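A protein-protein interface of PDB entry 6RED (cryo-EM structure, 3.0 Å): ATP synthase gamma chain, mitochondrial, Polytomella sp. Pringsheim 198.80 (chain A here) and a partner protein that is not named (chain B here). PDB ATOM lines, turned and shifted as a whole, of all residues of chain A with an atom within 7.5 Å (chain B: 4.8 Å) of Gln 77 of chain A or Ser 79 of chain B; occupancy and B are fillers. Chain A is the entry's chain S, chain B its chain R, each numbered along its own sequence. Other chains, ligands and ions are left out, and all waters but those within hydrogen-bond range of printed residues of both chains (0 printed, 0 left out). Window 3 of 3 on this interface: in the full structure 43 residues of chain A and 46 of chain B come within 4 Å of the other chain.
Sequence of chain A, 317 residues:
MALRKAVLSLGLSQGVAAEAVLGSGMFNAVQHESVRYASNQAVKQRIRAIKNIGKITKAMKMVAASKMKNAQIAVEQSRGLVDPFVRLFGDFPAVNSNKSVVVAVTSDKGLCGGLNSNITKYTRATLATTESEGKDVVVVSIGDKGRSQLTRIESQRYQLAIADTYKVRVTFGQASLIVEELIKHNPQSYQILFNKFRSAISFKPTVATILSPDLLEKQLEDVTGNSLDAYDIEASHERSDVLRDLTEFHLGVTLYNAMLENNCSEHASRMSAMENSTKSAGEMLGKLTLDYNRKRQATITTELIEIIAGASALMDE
Of the 7 printed residues of chain B, 6 touch a printed residue of chain A. Hydrophobic or aromatic side chains of chain B that line the printed part of chain A: Tyr 75, Pro 77 and Ile 80. Of the 14 printed residues of chain A, 6 touch a printed residue of chain B. Along chain A the printed residues that touch a printed residue of chain B span positions 76 to 256. Among the printed residues, 10 pairs touch across the chains.
The backbone NH of Ile 80 of chain B sits at hydrogen-bond distance from the side-chain amide oxygen of Gln 77 of chain A.
A ring nitrogen (NE2) of His 78 of chain B sits close to the side-chain hydroxyl (OG1) of Thr 76 of chain B, 3.5 Å away. O of Ala 74 of chain A lies within hydrogen-bond range of OG of Ser 78 of chain A, 3.4 Å away. O of Val 75 of chain A sits at hydrogen-bond distance from OG of Ser 78 of chain A (3.2 Å). The side-chain amide oxygen of Asn 257 of chain A sits at hydrogen-bond distance from the side-chain hydroxyl of Ser 78 of chain A. OG1 of Thr 76 of chain B lies within hydrogen-bond range of O of Ser 79 of chain B, at 2.5 Å.
Among the printed residues, pairs that only touch across the chains: Tyr 256 of chain A with Pro 77 of chain B (3.2 Å), Gly 80 of chain A with Tyr 75 of chain B (3.2 Å), Gln 77 of chain A with Ser 79 of chain B (3.3 Å), Gln 77 of chain A with His 78 of chain B (3.3 Å), Glu 76 of chain A with Ile 80 of chain B (3.5 Å), Ser 78 of chain A with Pro 77 of chain B (3.6 Å), Leu 81 of chain A with Pro 77 of chain B (3.7 Å), Leu 81 of chain A with Tyr 75 of chain B (3.7 Å) and Leu 81 of chain A with Thr 76 of chain B (3.9 Å).
Ile 73 of chain A touches none of the printed residues of chain B. Gln 77 of chain A touches just these residues of chain B: His 78 (3.3 Å), Ser 79 (3.3 Å) and Ile 80 (2.8 Å). Of the printed residues of chain B, Ser 78 of chain A touches Pro 77. Of the printed residues of chain B, Tyr 256 of chain A touches Pro 77. Asn 257 of chain A touches none of the printed residues of chain B. Of the printed residues of chain A, Pro 77 of chain B touches Ser 78, Leu 81 and Tyr 256. Printed residues of chain A within 4 Å of His 78 of chain B: Gln 77 (3.3 Å). Printed residues of chain A within 4 Å of Ile 80 of chain B: Glu 76 (3.5 Å) and Gln 77 (2.8 Å).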
ATOM      1  N   GLN A  72      28.747  14.904 -21.962  1.00  0.00           N
ATOM      2  CA  GLN A  72      29.345  16.106 -21.407  1.00  0.00           C
ATOM      3  C   GLN A  72      28.300  17.154 -21.063  1.00  0.00           C
ATOM      4  O   GLN A  72      28.420  17.839 -20.037  1.00  0.00           O
ATOM      5  CB  GLN A  72      30.338  16.684 -22.408  1.00  0.00           C
ATOM      6  CG  GLN A  72      31.199  17.796 -21.909  1.00  0.00           C
ATOM      7  CD  GLN A  72      32.218  18.198 -22.950  1.00  0.00           C
ATOM      8  OE1 GLN A  72      32.408  17.497 -23.940  1.00  0.00           O
ATOM      9  NE2 GLN A  72      32.875  19.329 -22.735  1.00  0.00           N
ATOM     10  N   ILE A  73      27.268  17.273 -21.902  1.00  0.00           N
ATOM     11  CA  ILE A  73      26.175  18.194 -21.629  1.00  0.00           C
ATOM     12  C   ILE A  73      25.388  17.757 -20.404  1.00  0.00           C
ATOM     13  O   ILE A  73      24.960  18.602 -19.616  1.00  0.00           O
ATOM     14  CB  ILE A  73      25.278  18.356 -22.874  1.00  0.00           C
ATOM     15  CG1 ILE A  73      24.768  17.009 -23.383  1.00  0.00           C
ATOM     16  CG2 ILE A  73      26.028  19.089 -23.975  1.00  0.00           C
ATOM     17  CD1 ILE A  73      23.744  17.130 -24.468  1.00  0.00           C
ATOM     18  N   ALA A  74      25.235  16.448 -20.187  1.00  0.00           N
ATOM     19  CA  ALA A  74      24.581  15.958 -18.981  1.00  0.00           C
ATOM     20  C   ALA A  74      25.392  16.280 -17.737  1.00  0.00           C
ATOM     21  O   ALA A  74      24.819  16.584 -16.683  1.00  0.00           O
ATOM     22  CB  ALA A  74      24.356  14.454 -19.087  1.00  0.00           C
ATOM     23  N   VAL A  75      26.716  16.260 -17.860  1.00  0.00           N
ATOM     24  CA  VAL A  75      27.597  16.607 -16.751  1.00  0.00           C
ATOM     25  C   VAL A  75      27.493  18.084 -16.422  1.00  0.00           C
ATOM     26  O   VAL A  75      27.428  18.463 -15.246  1.00  0.00           O
ATOM     27  CB  VAL A  75      29.034  16.191 -17.095  1.00  0.00           C
ATOM     28  CG1 VAL A  75      30.022  16.789 -16.151  1.00  0.00           C
ATOM     29  CG2 VAL A  75      29.123  14.722 -16.999  1.00  0.00           C
ATOM     30  N   GLU A  76      27.449  18.942 -17.440  1.00  0.00           N
ATOM     31  CA  GLU A  76      27.358  20.365 -17.141  1.00  0.00           C
ATOM     32  C   GLU A  76      25.969  20.732 -16.636  1.00  0.00           C
ATOM     33  O   GLU A  76      25.831  21.667 -15.844  1.00  0.00           O
ATOM     34  CB  GLU A  76      27.722  21.198 -18.365  1.00  0.00           C
ATOM     35  CG  GLU A  76      28.330  22.579 -18.044  1.00  0.00           C
ATOM     36  CD  GLU A  76      27.320  23.660 -17.690  1.00  0.00           C
ATOM     37  OE1 GLU A  76      26.155  23.577 -18.127  1.00  0.00           O
ATOM     38  OE2 GLU A  76      27.703  24.608 -16.980  1.00  0.00           O
ATOM     39  N   GLN A  77      24.937  19.995 -17.054  1.00  0.00           N
ATOM     40  CA  GLN A  77      23.601  20.251 -16.530  1.00  0.00           C
ATOM     41  C   GLN A  77      23.478  19.800 -15.083  1.00  0.00           C
ATOM     42  O   GLN A  77      22.833  20.476 -14.276  1.00  0.00           O
ATOM     43  CB  GLN A  77      22.545  19.560 -17.386  1.00  0.00           C
ATOM     44  CG  GLN A  77      22.302  20.187 -18.742  1.00  0.00           C
ATOM     45  CD  GLN A  77      22.032  21.671 -18.693  1.00  0.00           C
ATOM     46  OE1 GLN A  77      20.965  22.105 -18.272  1.00  0.00           O
ATOM     47  NE2 GLN A  77      22.993  22.461 -19.146  1.00  0.00           N
ATOM     48  N   SER A  78      24.090  18.676 -14.724  1.00  0.00           N
ATOM     49  CA  SER A  78      23.985  18.230 -13.340  1.00  0.00           C
ATOM     50  C   SER A  78      24.881  19.007 -12.393  1.00  0.00           C
ATOM     51  O   SER A  78      24.748  18.854 -11.180  1.00  0.00           O
ATOM     52  CB  SER A  78      24.330  16.755 -13.221  1.00  0.00           C
ATOM     53  OG  SER A  78      25.715  16.560 -13.403  1.00  0.00           O
ATOM     54  N   ARG A  79      25.787  19.832 -12.912  1.00  0.00           N
ATOM     55  CA  ARG A  79      26.680  20.626 -12.084  1.00  0.00           C
ATOM     56  C   ARG A  79      25.971  21.753 -11.363  1.00  0.00           C
ATOM     57  O   ARG A  79      26.555  22.346 -10.458  1.00  0.00           O
ATOM     58  CB  ARG A  79      27.784  21.233 -12.942  1.00  0.00           C
ATOM     59  CG  ARG A  79      29.130  20.576 -12.849  1.00  0.00           C
ATOM     60  CD  ARG A  79      29.883  20.831 -14.129  1.00  0.00           C
ATOM     61  NE  ARG A  79      31.309  20.575 -14.001  1.00  0.00           N
ATOM     62  CZ  ARG A  79      32.111  20.310 -15.025  1.00  0.00           C
ATOM     63  NH1 ARG A  79      31.621  20.251 -16.254  1.00  0.00           N
ATOM     64  NH2 ARG A  79      33.400  20.099 -14.818  1.00  0.00           N
ATOM     65  N   GLY A  80      24.752  22.092 -11.769  1.00  0.00           N
ATOM     66  CA  GLY A  80      24.080  23.220 -11.160  1.00  0.00           C
ATOM     67  C   GLY A  80      23.539  22.901  -9.782  1.00  0.00           C
ATOM     68  O   GLY A  80      23.676  23.700  -8.858  1.00  0.00           O
ATOM     69  N   LEU A  81      22.941  21.723  -9.621  1.00  0.00           N
ATOM     70  CA  LEU A  81      22.214  21.431  -8.393  1.00  0.00           C
ATOM     71  C   LEU A  81      23.137  21.174  -7.212  1.00  0.00           C
ATOM     72  O   LEU A  81      22.701  21.289  -6.067  1.00  0.00           O
ATOM     73  CB  LEU A  81      21.273  20.248  -8.617  1.00  0.00           C
ATOM     74  CG  LEU A  81      20.244  19.869  -7.554  1.00  0.00           C
ATOM     75  CD1 LEU A  81      19.527  21.073  -7.057  1.00  0.00           C
ATOM     76  CD2 LEU A  81      19.247  18.937  -8.131  1.00  0.00           C
ATOM     77  N   VAL A  82      24.412  20.864  -7.447  1.00  0.00           N
ATOM     78  CA  VAL A  82      25.288  20.600  -6.310  1.00  0.00           C
ATOM     79  C   VAL A  82      25.690  21.860  -5.573  1.00  0.00           C
ATOM     80  O   VAL A  82      26.053  21.779  -4.396  1.00  0.00           O
ATOM     81  CB  VAL A  82      26.571  19.850  -6.713  1.00  0.00           C
ATOM     82  CG1 VAL A  82      26.233  18.488  -7.201  1.00  0.00           C
ATOM     83  CG2 VAL A  82      27.316  20.590  -7.778  1.00  0.00           C
ATOM     84  N   TYR A 256      24.725  11.530  -7.663  1.00  0.00           N
ATOM     85  CA  TYR A 256      24.365  11.633  -9.071  1.00  0.00           C
ATOM     86  C   TYR A 256      25.438  12.365  -9.857  1.00  0.00           C
ATOM     87  O   TYR A 256      25.939  11.860 -10.869  1.00  0.00           O
ATOM     88  CB  TYR A 256      23.027  12.351  -9.190  1.00  0.00           C
ATOM     89  CG  TYR A 256      22.559  12.581 -10.589  1.00  0.00           C
ATOM     90  CD1 TYR A 256      22.089  11.541 -11.360  1.00  0.00           C
ATOM     91  CD2 TYR A 256      22.568  13.839 -11.135  1.00  0.00           C
ATOM     92  CE1 TYR A 256      21.656  11.755 -12.639  1.00  0.00           C
ATOM     93  CE2 TYR A 256      22.142  14.054 -12.408  1.00  0.00           C
ATOM     94  CZ  TYR A 256      21.692  13.013 -13.157  1.00  0.00           C
ATOM     95  OH  TYR A 256      21.257  13.236 -14.434  1.00  0.00           O
ATOM     96  N   ASN A 257      25.838  13.540  -9.374  1.00  0.00           N
ATOM     97  CA  ASN A 257      26.885  14.289 -10.051  1.00  0.00           C
ATOM     98  C   ASN A 257      28.233  13.600  -9.964  1.00  0.00           C
ATOM     99  O   ASN A 257      29.034  13.723 -10.886  1.00  0.00           O
ATOM    100  CB  ASN A 257      27.003  15.681  -9.470  1.00  0.00           C
ATOM    101  CG  ASN A 257      27.939  16.532 -10.247  1.00  0.00           C
ATOM    102  OD1 ASN A 257      27.948  16.492 -11.466  1.00  0.00           O
ATOM    103  ND2 ASN A 257      28.757  17.299  -9.550  1.00  0.00           N
ATOM    104  N   LEU A 260      28.208  10.862 -12.571  1.00  0.00           N
ATOM    105  CA  LEU A 260      28.094  11.440 -13.902  1.00  0.00           C
ATOM    106  C   LEU A 260      29.404  12.097 -14.347  1.00  0.00           C
ATOM    107  O   LEU A 260      29.863  11.880 -15.480  1.00  0.00           O
ATOM    108  CB  LEU A 260      26.916  12.410 -13.906  1.00  0.00           C
ATOM    109  CG  LEU A 260      26.363  12.970 -15.196  1.00  0.00           C
ATOM    110  CD1 LEU A 260      26.256  11.887 -16.212  1.00  0.00           C
ATOM    111  CD2 LEU A 260      25.004  13.484 -14.906  1.00  0.00           C
ATOM    112  N   TYR B  75      16.755  24.823 -10.537  1.00  0.00           N
ATOM    113  CA  TYR B  75      17.582  23.651 -10.785  1.00  0.00           C
ATOM    114  C   TYR B  75      16.773  22.367 -10.779  1.00  0.00           C
ATOM    115  O   TYR B  75      15.810  22.224 -10.030  1.00  0.00           O
ATOM    116  CB  TYR B  75      18.666  23.512  -9.739  1.00  0.00           C
ATOM    117  CG  TYR B  75      19.786  24.493  -9.862  1.00  0.00           C
ATOM    118  CD1 TYR B  75      20.291  24.849 -11.098  1.00  0.00           C
ATOM    119  CD2 TYR B  75      20.349  25.060  -8.734  1.00  0.00           C
ATOM    120  CE1 TYR B  75      21.324  25.747 -11.207  1.00  0.00           C
ATOM    121  CE2 TYR B  75      21.377  25.955  -8.834  1.00  0.00           C
ATOM    122  CZ  TYR B  75      21.862  26.294 -10.072  1.00  0.00           C
ATOM    123  OH  TYR B  75      22.892  27.195 -10.165  1.00  0.00           O
ATOM    124  N   THR B  76      17.190  21.442 -11.620  1.00  0.00           N
ATOM    125  CA  THR B  76      16.782  20.049 -11.654  1.00  0.00           C
ATOM    126  C   THR B  76      18.046  19.218 -11.782  1.00  0.00           C
ATOM    127  O   THR B  76      19.094  19.743 -12.169  1.00  0.00           O
ATOM    128  CB  THR B  76      15.832  19.775 -12.826  1.00  0.00           C
ATOM    129  OG1 THR B  76      16.407  20.281 -14.033  1.00  0.00           O
ATOM    130  CG2 THR B  76      14.489  20.396 -12.587  1.00  0.00           C
ATOM    131  N   PRO B  77      18.002  17.932 -11.425  1.00  0.00           N
ATOM    132  CA  PRO B  77      19.190  17.093 -11.639  1.00  0.00           C
ATOM    133  C   PRO B  77      19.559  16.907 -13.099  1.00  0.00           C
ATOM    134  O   PRO B  77      20.731  16.688 -13.414  1.00  0.00           O
ATOM    135  CB  PRO B  77      18.788  15.765 -10.998  1.00  0.00           C
ATOM    136  CG  PRO B  77      17.795  16.121 -10.003  1.00  0.00           C
ATOM    137  CD  PRO B  77      17.032  17.263 -10.545  1.00  0.00           C
ATOM    138  N   HIS B  78      18.602  17.012 -14.008  1.00  0.00           N
ATOM    139  CA  HIS B  78      18.862  16.804 -15.418  1.00  0.00           C
ATOM    140  C   HIS B  78      19.076  18.092 -16.190  1.00  0.00           C
ATOM    141  O   HIS B  78      19.576  18.034 -17.315  1.00  0.00           O
ATOM    142  CB  HIS B  78      17.697  16.049 -16.040  1.00  0.00           C
ATOM    143  CG  HIS B  78      16.369  16.562 -15.601  1.00  0.00           C
ATOM    144  ND1 HIS B  78      15.688  16.036 -14.527  1.00  0.00           N
ATOM    145  CD2 HIS B  78      15.612  17.581 -16.066  1.00  0.00           C
ATOM    146  CE1 HIS B  78      14.559  16.697 -14.360  1.00  0.00           C
ATOM    147  NE2 HIS B  78      14.488  17.640 -15.281  1.00  0.00           N
ATOM    148  N   SER B  79      18.712  19.240 -15.633  1.00  0.00           N
ATOM    149  CA  SER B  79      18.744  20.463 -16.416  1.00  0.00           C
ATOM    150  C   SER B  79      18.852  21.664 -15.500  1.00  0.00           C
ATOM    151  O   SER B  79      18.488  21.600 -14.328  1.00  0.00           O
ATOM    152  CB  SER B  79      17.498  20.605 -17.285  1.00  0.00           C
ATOM    153  OG  SER B  79      16.388  20.965 -16.490  1.00  0.00           O
ATOM    154  N   ILE B  80      19.351  22.755 -16.060  1.00  0.00           N
ATOM    155  CA  ILE B  80      19.451  24.036 -15.380  1.00  0.00           C
ATOM    156  C   ILE B  80      18.437  24.957 -16.029  1.00  0.00           C
ATOM    157  O   ILE B  80      18.647  25.441 -17.144  1.00  0.00           O
ATOM    158  CB  ILE B  80      20.868  24.609 -15.467  1.00  0.00           C
ATOM    159  CG1 ILE B  80      21.856  23.637 -14.830  1.00  0.00           C
ATOM    160  CG2 ILE B  80      20.935  25.947 -14.795  1.00  0.00           C
ATOM    161  CD1 ILE B  80      23.289  24.003 -15.021  1.00  0.00           C
ATOM    162  N   LEU B  81      17.332  25.203 -15.335  1.00  0.00           N
ATOM    163  CA  LEU B  81      16.173  25.820 -15.961  1.00  0.00           C
ATOM    164  C   LEU B  81      16.270  27.329 -16.054  1.00  0.00           C
ATOM    165  O   LEU B  81      15.773  27.908 -17.024  1.00  0.00           O
ATOM    166  CB  LEU B  81      14.917  25.425 -15.198  1.00  0.00           C
ATOM    167  CG  LEU B  81      14.638  23.947 -15.405  1.00  0.00           C
ATOM    168  CD1 LEU B  81      13.631  23.475 -14.439  1.00  0.00           C
ATOM    169  CD2 LEU B  81      14.116  23.768 -16.804  1.00  0.00           C
